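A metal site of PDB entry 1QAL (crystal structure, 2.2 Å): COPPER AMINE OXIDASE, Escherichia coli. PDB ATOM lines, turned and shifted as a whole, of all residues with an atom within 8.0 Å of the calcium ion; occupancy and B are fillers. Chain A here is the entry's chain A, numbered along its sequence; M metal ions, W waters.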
ATOM      1  N   LYS A 128      25.891 -13.270  38.155  1.00  0.00           N
ATOM      2  CA  LYS A 128      25.614 -14.571  37.588  1.00  0.00           C
ATOM      3  C   LYS A 128      26.722 -15.596  37.843  1.00  0.00           C
ATOM      4  O   LYS A 128      26.471 -16.780  38.164  1.00  0.00           O
ATOM      5  CB  LYS A 128      25.399 -14.353  36.066  1.00  0.00           C
ATOM      6  CG  LYS A 128      25.480 -15.602  35.190  1.00  0.00           C
ATOM      7  CD  LYS A 128      24.881 -15.231  33.828  1.00  0.00           C
ATOM      8  CE  LYS A 128      24.877 -16.422  32.886  1.00  0.00           C
ATOM      9  NZ  LYS A 128      24.083 -16.035  31.676  1.00  0.00           N
ATOM     10  N   TRP A 132      26.365 -19.301  39.591  1.00  0.00           N
ATOM     11  CA  TRP A 132      26.677 -20.603  38.982  1.00  0.00           C
ATOM     12  C   TRP A 132      27.723 -21.341  39.828  1.00  0.00           C
ATOM     13  O   TRP A 132      27.590 -22.565  39.974  1.00  0.00           O
ATOM     14  CB  TRP A 132      27.205 -20.417  37.546  1.00  0.00           C
ATOM     15  CG  TRP A 132      26.237 -20.506  36.423  1.00  0.00           C
ATOM     16  CD1 TRP A 132      26.078 -19.624  35.383  1.00  0.00           C
ATOM     17  CD2 TRP A 132      25.264 -21.540  36.179  1.00  0.00           C
ATOM     18  NE1 TRP A 132      25.081 -20.019  34.499  1.00  0.00           N
ATOM     19  CE2 TRP A 132      24.575 -21.203  35.004  1.00  0.00           C
ATOM     20  CE3 TRP A 132      24.925 -22.703  36.875  1.00  0.00           C
ATOM     21  CZ2 TRP A 132      23.542 -21.995  34.467  1.00  0.00           C
ATOM     22  CZ3 TRP A 132      23.906 -23.507  36.368  1.00  0.00           C
ATOM     23  CH2 TRP A 132      23.260 -23.122  35.186  1.00  0.00           C
ATOM     24  N   VAL A 351      22.395 -25.480  31.342  1.00  0.00           N
ATOM     25  CA  VAL A 351      21.396 -25.411  30.296  1.00  0.00           C
ATOM     26  C   VAL A 351      20.825 -23.997  30.312  1.00  0.00           C
ATOM     27  O   VAL A 351      20.779 -23.269  29.314  1.00  0.00           O
ATOM     28  CB  VAL A 351      20.268 -26.424  30.531  1.00  0.00           C
ATOM     29  CG1 VAL A 351      19.178 -26.268  29.472  1.00  0.00           C
ATOM     30  CG2 VAL A 351      20.867 -27.812  30.446  1.00  0.00           C
ATOM     31  N   MET A 352      20.369 -23.566  31.493  1.00  0.00           N
ATOM     32  CA  MET A 352      19.784 -22.235  31.602  1.00  0.00           C
ATOM     33  C   MET A 352      20.064 -21.560  32.930  1.00  0.00           C
ATOM     34  O   MET A 352      19.838 -22.051  34.053  1.00  0.00           O
ATOM     35  CB  MET A 352      18.233 -22.355  31.492  1.00  0.00           C
ATOM     36  CG  MET A 352      17.498 -21.014  31.382  1.00  0.00           C
ATOM     37  SD  MET A 352      15.755 -21.094  30.855  1.00  0.00           S
ATOM     38  CE  MET A 352      15.100 -22.176  32.130  1.00  0.00           C
ATOM     39  N   TYR A 353      20.577 -20.337  32.873  1.00  0.00           N
ATOM     40  CA  TYR A 353      20.841 -19.588  34.103  1.00  0.00           C
ATOM     41  C   TYR A 353      19.528 -19.103  34.687  1.00  0.00           C
ATOM     42  O   TYR A 353      19.232 -19.238  35.869  1.00  0.00           O
ATOM     43  CB  TYR A 353      21.793 -18.383  33.828  1.00  0.00           C
ATOM     44  CG  TYR A 353      21.952 -17.639  35.142  1.00  0.00           C
ATOM     45  CD1 TYR A 353      22.622 -18.229  36.197  1.00  0.00           C
ATOM     46  CD2 TYR A 353      21.437 -16.356  35.342  1.00  0.00           C
ATOM     47  CE1 TYR A 353      22.794 -17.569  37.425  1.00  0.00           C
ATOM     48  CE2 TYR A 353      21.593 -15.681  36.549  1.00  0.00           C
ATOM     49  CZ  TYR A 353      22.281 -16.303  37.577  1.00  0.00           C
ATOM     50  OH  TYR A 353      22.422 -15.644  38.764  1.00  0.00           O
ATOM     51  N   GLU A 354      18.673 -18.478  33.867  1.00  0.00           N
ATOM     52  CA  GLU A 354      17.377 -17.999  34.348  1.00  0.00           C
ATOM     53  C   GLU A 354      16.344 -17.982  33.235  1.00  0.00           C
ATOM     54  O   GLU A 354      16.658 -17.631  32.099  1.00  0.00           O
ATOM     55  CB  GLU A 354      17.301 -16.562  34.881  1.00  0.00           C
ATOM     56  CG  GLU A 354      18.349 -16.210  35.927  1.00  0.00           C
ATOM     57  CD  GLU A 354      18.168 -14.759  36.383  1.00  0.00           C
ATOM     58  OE1 GLU A 354      17.186 -14.614  37.137  1.00  0.00           O
ATOM     59  OE2 GLU A 354      18.912 -13.815  36.040  1.00  0.00           O
ATOM     60  N   ARG A 526      11.592 -14.827  28.658  1.00  0.00           N
ATOM     61  CA  ARG A 526      12.992 -14.417  28.708  1.00  0.00           C
ATOM     62  C   ARG A 526      13.781 -15.643  29.163  1.00  0.00           C
ATOM     63  O   ARG A 526      13.601 -15.980  30.341  1.00  0.00           O
ATOM     64  CB  ARG A 526      13.217 -13.217  29.639  1.00  0.00           C
ATOM     65  CG  ARG A 526      14.706 -12.946  29.864  1.00  0.00           C
ATOM     66  CD  ARG A 526      14.878 -11.807  30.881  1.00  0.00           C
ATOM     67  NE  ARG A 526      16.285 -11.371  30.945  1.00  0.00           N
ATOM     68  CZ  ARG A 526      17.157 -12.132  31.623  1.00  0.00           C
ATOM     69  NH1 ARG A 526      16.744 -13.263  32.210  1.00  0.00           N
ATOM     70  NH2 ARG A 526      18.426 -11.775  31.702  1.00  0.00           N
ATOM     71  N   LEU A 527      14.564 -16.212  28.273  1.00  0.00           N
ATOM     72  CA  LEU A 527      15.344 -17.373  28.603  1.00  0.00           C
ATOM     73  C   LEU A 527      16.848 -17.158  28.456  1.00  0.00           C
ATOM     74  O   LEU A 527      17.441 -17.248  27.371  1.00  0.00           O
ATOM     75  CB  LEU A 527      14.913 -18.567  27.670  1.00  0.00           C
ATOM     76  CG  LEU A 527      13.372 -18.615  27.437  1.00  0.00           C
ATOM     77  CD1 LEU A 527      13.034 -19.530  26.260  1.00  0.00           C
ATOM     78  CD2 LEU A 527      12.812 -19.132  28.768  1.00  0.00           C
ATOM     79  N   ASP A 528      17.467 -16.914  29.605  1.00  0.00           N
ATOM     80  CA  ASP A 528      18.934 -16.753  29.601  1.00  0.00           C
ATOM     81  C   ASP A 528      19.558 -18.151  29.582  1.00  0.00           C
ATOM     82  O   ASP A 528      20.068 -18.695  30.578  1.00  0.00           O
ATOM     83  CB  ASP A 528      19.401 -16.016  30.845  1.00  0.00           C
ATOM     84  CG  ASP A 528      20.896 -15.927  30.974  1.00  0.00           C
ATOM     85  OD1 ASP A 528      21.673 -16.205  30.062  1.00  0.00           O
ATOM     86  OD2 ASP A 528      21.428 -15.584  32.019  1.00  0.00           O
ATOM     87  N   LEU A 529      19.536 -18.754  28.372  1.00  0.00           N
ATOM     88  CA  LEU A 529      20.109 -20.077  28.191  1.00  0.00           C
ATOM     89  C   LEU A 529      21.649 -20.016  28.189  1.00  0.00           C
ATOM     90  O   LEU A 529      22.092 -19.102  27.536  1.00  0.00           O
ATOM     91  CB  LEU A 529      19.660 -20.602  26.796  1.00  0.00           C
ATOM     92  CG  LEU A 529      18.157 -20.943  26.704  1.00  0.00           C
ATOM     93  CD1 LEU A 529      17.749 -21.182  25.257  1.00  0.00           C
ATOM     94  CD2 LEU A 529      17.768 -22.071  27.670  1.00  0.00           C
ATOM     95  N   ASP A 530      22.337 -20.932  28.865  1.00  0.00           N
ATOM     96  CA  ASP A 530      23.801 -20.944  28.880  1.00  0.00           C
ATOM     97  C   ASP A 530      24.006 -22.410  28.447  1.00  0.00           C
ATOM     98  O   ASP A 530      24.017 -23.281  29.301  1.00  0.00           O
ATOM     99  CB  ASP A 530      24.418 -20.723  30.235  1.00  0.00           C
ATOM    100  CG  ASP A 530      24.334 -19.300  30.759  1.00  0.00           C
ATOM    101  OD1 ASP A 530      24.059 -18.292  30.081  1.00  0.00           O
ATOM    102  OD2 ASP A 530      24.575 -19.140  31.972  1.00  0.00           O
ATOM    103  N   VAL A 531      24.126 -22.629  27.120  1.00  0.00           N
ATOM    104  CA  VAL A 531      24.276 -23.977  26.617  1.00  0.00           C
ATOM    105  C   VAL A 531      25.608 -24.611  26.918  1.00  0.00           C
ATOM    106  O   VAL A 531      26.534 -24.303  26.167  1.00  0.00           O
ATOM    107  CB  VAL A 531      23.940 -23.960  25.127  1.00  0.00           C
ATOM    108  CG1 VAL A 531      24.198 -25.320  24.492  1.00  0.00           C
ATOM    109  CG2 VAL A 531      22.483 -23.517  24.920  1.00  0.00           C
ATOM    110  N   GLY A 533      27.575 -23.877  28.909  1.00  0.00           N
ATOM    111  CA  GLY A 533      28.587 -22.851  29.199  1.00  0.00           C
ATOM    112  C   GLY A 533      28.040 -21.480  28.886  1.00  0.00           C
ATOM    113  O   GLY A 533      26.932 -21.367  28.333  1.00  0.00           O
ATOM    114  N   GLU A 534      28.810 -20.473  29.274  1.00  0.00           N
ATOM    115  CA  GLU A 534      28.438 -19.069  29.038  1.00  0.00           C
ATOM    116  C   GLU A 534      28.416 -18.560  27.601  1.00  0.00           C
ATOM    117  O   GLU A 534      27.454 -18.004  27.075  1.00  0.00           O
ATOM    118  CB  GLU A 534      29.417 -18.176  29.819  1.00  0.00           C
ATOM    119  CG  GLU A 534      29.049 -16.701  29.844  1.00  0.00           C
ATOM    120  CD  GLU A 534      30.194 -15.825  30.346  1.00  0.00           C
ATOM    121  OE1 GLU A 534      31.010 -16.246  31.190  1.00  0.00           O
ATOM    122  OE2 GLU A 534      30.302 -14.672  29.901  1.00  0.00           O
ATOM    123  N   ASN A 535      29.519 -18.739  26.902  1.00  0.00           N
ATOM    124  CA  ASN A 535      29.738 -18.292  25.529  1.00  0.00           C
ATOM    125  C   ASN A 535      29.100 -19.150  24.472  1.00  0.00           C
ATOM    126  O   ASN A 535      29.530 -20.275  24.279  1.00  0.00           O
ATOM    127  CB  ASN A 535      31.268 -18.155  25.287  1.00  0.00           C
ATOM    128  CG  ASN A 535      31.890 -17.304  26.408  1.00  0.00           C
ATOM    129  OD1 ASN A 535      31.364 -16.270  26.775  1.00  0.00           O
ATOM    130  ND2 ASN A 535      33.009 -17.623  27.041  1.00  0.00           N
ATOM    131  N   ASN A 536      28.083 -18.620  23.799  1.00  0.00           N
ATOM    132  CA  ASN A 536      27.342 -19.310  22.773  1.00  0.00           C
ATOM    133  C   ASN A 536      27.195 -18.436  21.530  1.00  0.00           C
ATOM    134  O   ASN A 536      27.584 -17.276  21.629  1.00  0.00           O
ATOM    135  CB  ASN A 536      25.897 -19.669  23.252  1.00  0.00           C
ATOM    136  CG  ASN A 536      25.929 -20.439  24.581  1.00  0.00           C
ATOM    137  OD1 ASN A 536      26.911 -21.090  24.993  1.00  0.00           O
ATOM    138  ND2 ASN A 536      24.775 -20.353  25.278  1.00  0.00           N
ATOM    139  N   LEU A 583      20.982 -22.373  19.539  1.00  0.00           N
ATOM    140  CA  LEU A 583      21.848 -21.560  20.398  1.00  0.00           C
ATOM    141  C   LEU A 583      22.891 -22.683  20.629  1.00  0.00           C
ATOM    142  O   LEU A 583      22.594 -23.660  21.321  1.00  0.00           O
ATOM    143  CB  LEU A 583      21.254 -20.969  21.670  1.00  0.00           C
ATOM    144  CG  LEU A 583      22.309 -20.189  22.481  1.00  0.00           C
ATOM    145  CD1 LEU A 583      22.662 -18.911  21.725  1.00  0.00           C
ATOM    146  CD2 LEU A 583      21.823 -19.782  23.861  1.00  0.00           C
ATOM    147  N   THR A 636      19.716 -11.344  22.682  1.00  0.00           N
ATOM    148  CA  THR A 636      20.517 -10.192  23.068  1.00  0.00           C
ATOM    149  C   THR A 636      21.660 -10.622  23.968  1.00  0.00           C
ATOM    150  O   THR A 636      21.609 -11.748  24.473  1.00  0.00           O
ATOM    151  CB  THR A 636      19.687  -9.148  23.846  1.00  0.00           C
ATOM    152  OG1 THR A 636      19.119  -9.751  25.053  1.00  0.00           O
ATOM    153  CG2 THR A 636      18.569  -8.653  22.928  1.00  0.00           C
ATOM    154  N   ARG A 637      22.614  -9.714  24.090  1.00  0.00           N
ATOM    155  CA  ARG A 637      23.814  -9.895  24.923  1.00  0.00           C
ATOM    156  C   ARG A 637      23.315  -9.837  26.364  1.00  0.00           C
ATOM    157  O   ARG A 637      22.511  -8.957  26.649  1.00  0.00           O
ATOM    158  CB  ARG A 637      24.748  -8.730  24.559  1.00  0.00           C
ATOM    159  CG  ARG A 637      25.986  -8.717  25.440  1.00  0.00           C
ATOM    160  CD  ARG A 637      26.906  -9.822  24.994  1.00  0.00           C
ATOM    161  NE  ARG A 637      28.275  -9.486  24.646  1.00  0.00           N
ATOM    162  CZ  ARG A 637      28.480  -8.680  23.598  1.00  0.00           C
ATOM    163  NH1 ARG A 637      27.435  -8.245  22.919  1.00  0.00           N
ATOM    164  NH2 ARG A 637      29.781  -8.561  23.522  1.00  0.00           N
ATOM    165  N   TYR A 638      23.694 -10.710  27.272  1.00  0.00           N
ATOM    166  CA  TYR A 638      23.265 -10.745  28.645  1.00  0.00           C
ATOM    167  C   TYR A 638      23.673  -9.440  29.343  1.00  0.00           C
ATOM    168  O   TYR A 638      24.815  -8.990  29.234  1.00  0.00           O
ATOM    169  CB  TYR A 638      23.878 -11.941  29.416  1.00  0.00           C
ATOM    170  CG  TYR A 638      23.663 -11.780  30.915  1.00  0.00           C
ATOM    171  CD1 TYR A 638      22.423 -12.028  31.517  1.00  0.00           C
ATOM    172  CD2 TYR A 638      24.705 -11.376  31.742  1.00  0.00           C
ATOM    173  CE1 TYR A 638      22.199 -11.890  32.890  1.00  0.00           C
ATOM    174  CE2 TYR A 638      24.507 -11.226  33.096  1.00  0.00           C
ATOM    175  CZ  TYR A 638      23.272 -11.481  33.679  1.00  0.00           C
ATOM    176  OH  TYR A 638      23.153 -11.311  35.046  1.00  0.00           O
ATOM    177  N   THR A 672      29.389 -15.513  22.787  1.00  0.00           N
ATOM    178  CA  THR A 672      29.212 -14.661  23.962  1.00  0.00           C
ATOM    179  C   THR A 672      27.970 -15.073  24.734  1.00  0.00           C
ATOM    180  O   THR A 672      27.129 -15.896  24.336  1.00  0.00           O
ATOM    181  CB  THR A 672      29.165 -13.193  23.469  1.00  0.00           C
ATOM    182  OG1 THR A 672      29.207 -12.324  24.596  1.00  0.00           O
ATOM    183  CG2 THR A 672      28.018 -12.878  22.545  1.00  0.00           C
ATOM    184  N   ASP A 673      27.805 -14.478  25.909  1.00  0.00           N
ATOM    185  CA  ASP A 673      26.672 -14.770  26.775  1.00  0.00           C
ATOM    186  C   ASP A 673      25.381 -14.248  26.164  1.00  0.00           C
ATOM    187  O   ASP A 673      25.077 -13.055  26.190  1.00  0.00           O
ATOM    188  CB  ASP A 673      26.925 -14.297  28.215  1.00  0.00           C
ATOM    189  CG  ASP A 673      25.819 -14.794  29.142  1.00  0.00           C
ATOM    190  OD1 ASP A 673      24.777 -15.373  28.754  1.00  0.00           O
ATOM    191  OD2 ASP A 673      25.978 -14.596  30.352  1.00  0.00           O
ATOM    192  N   ALA A 674      24.558 -15.099  25.540  1.00  0.00           N
ATOM    193  CA  ALA A 674      23.310 -14.682  24.881  1.00  0.00           C
ATOM    194  C   ALA A 674      22.111 -14.938  25.804  1.00  0.00           C
ATOM    195  O   ALA A 674      22.099 -15.770  26.704  1.00  0.00           O
ATOM    196  CB  ALA A 674      23.027 -15.567  23.652  1.00  0.00           C
ATOM    197  N   VAL A 675      21.049 -14.226  25.578  1.00  0.00           N
ATOM    198  CA  VAL A 675      19.775 -14.314  26.265  1.00  0.00           C
ATOM    199  C   VAL A 675      18.742 -14.406  25.116  1.00  0.00           C
ATOM    200  O   VAL A 675      18.688 -13.529  24.270  1.00  0.00           O
ATOM    201  CB  VAL A 675      19.432 -13.062  27.116  1.00  0.00           C
ATOM    202  CG1 VAL A 675      17.982 -13.193  27.608  1.00  0.00           C
ATOM    203  CG2 VAL A 675      20.327 -12.936  28.359  1.00  0.00           C
ATOM    204  N   VAL A 676      17.936 -15.438  25.102  1.00  0.00           N
ATOM    205  CA  VAL A 676      16.921 -15.666  24.085  1.00  0.00           C
ATOM    206  C   VAL A 676      15.566 -15.192  24.596  1.00  0.00           C
ATOM    207  O   VAL A 676      15.261 -15.381  25.773  1.00  0.00           O
ATOM    208  CB  VAL A 676      16.824 -17.185  23.823  1.00  0.00           C
ATOM    209  CG1 VAL A 676      15.664 -17.459  22.850  1.00  0.00           C
ATOM    210  CG2 VAL A 676      18.185 -17.684  23.333  1.00  0.00           C
HETATM  211 CA    CA M   1      23.101 -16.993  28.368  1.00  0.00          CA
HETATM  212  O   HOH W   1      24.881 -17.917  26.553  1.00  0.00           O
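Water W1 lies within hydrogen-bond range of O of Glu 534 (2.6 Å), ND2 of Asn 536 (2.8 Å) and N of Ala 674 (3.0 Å).
The backbone NH of Tyr 353 is in hydrogen-bond range of the backbone carbonyl oxygen of Asp 528, 2.9 Å away. NZ of Lys 128 is in salt-bridge range of OD2 of Asp 530. N of Asp 530 lies within hydrogen-bond range of O of Val 351, at 2.8 Å. The backbone carbonyl oxygen (O) of Asp 673 lies within hydrogen-bond range of the backbone NH (N) of Tyr 638. The backbone NH (N) of Asp 528 is in hydrogen-bond range of the backbone carbonyl oxygen (O) of Glu 354 (2.7 Å). NZ of Lys 128 lies within salt-bridge range of OD2 of Asp 528 (2.7 Å). The side-chain carboxylate (OD2) of Asp 530 sits at hydrogen-bond distance from the indole nitrogen (NE1) of Trp 132 (2.7 Å). OD2 of Asp 673 lies within salt-bridge range of NZ of Lys 128, at 2.7 Å.
Residues that only touch the calcium ion: Lys 128 (3.6 Å). Within 4 Å of the calcium ion: Lys 128, Asp 528, Leu 529, Asp 530, Asp 673 and Ala 674.
O of Ala 674 binds the calcium ion (2.3 Å). The calcium ion is bound by the side-chain carboxylate (OD1) of Asp 528. The calcium ion is bound by OD1 of Asp 530 (2.4 Å). The calcium ion is bound by the side-chain carboxylate (OD1) of Asp 673. O of Leu 529 is bound to the calcium ion (2.5 Å). Water W1 is bound to the calcium ion, at 2.7 Å.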
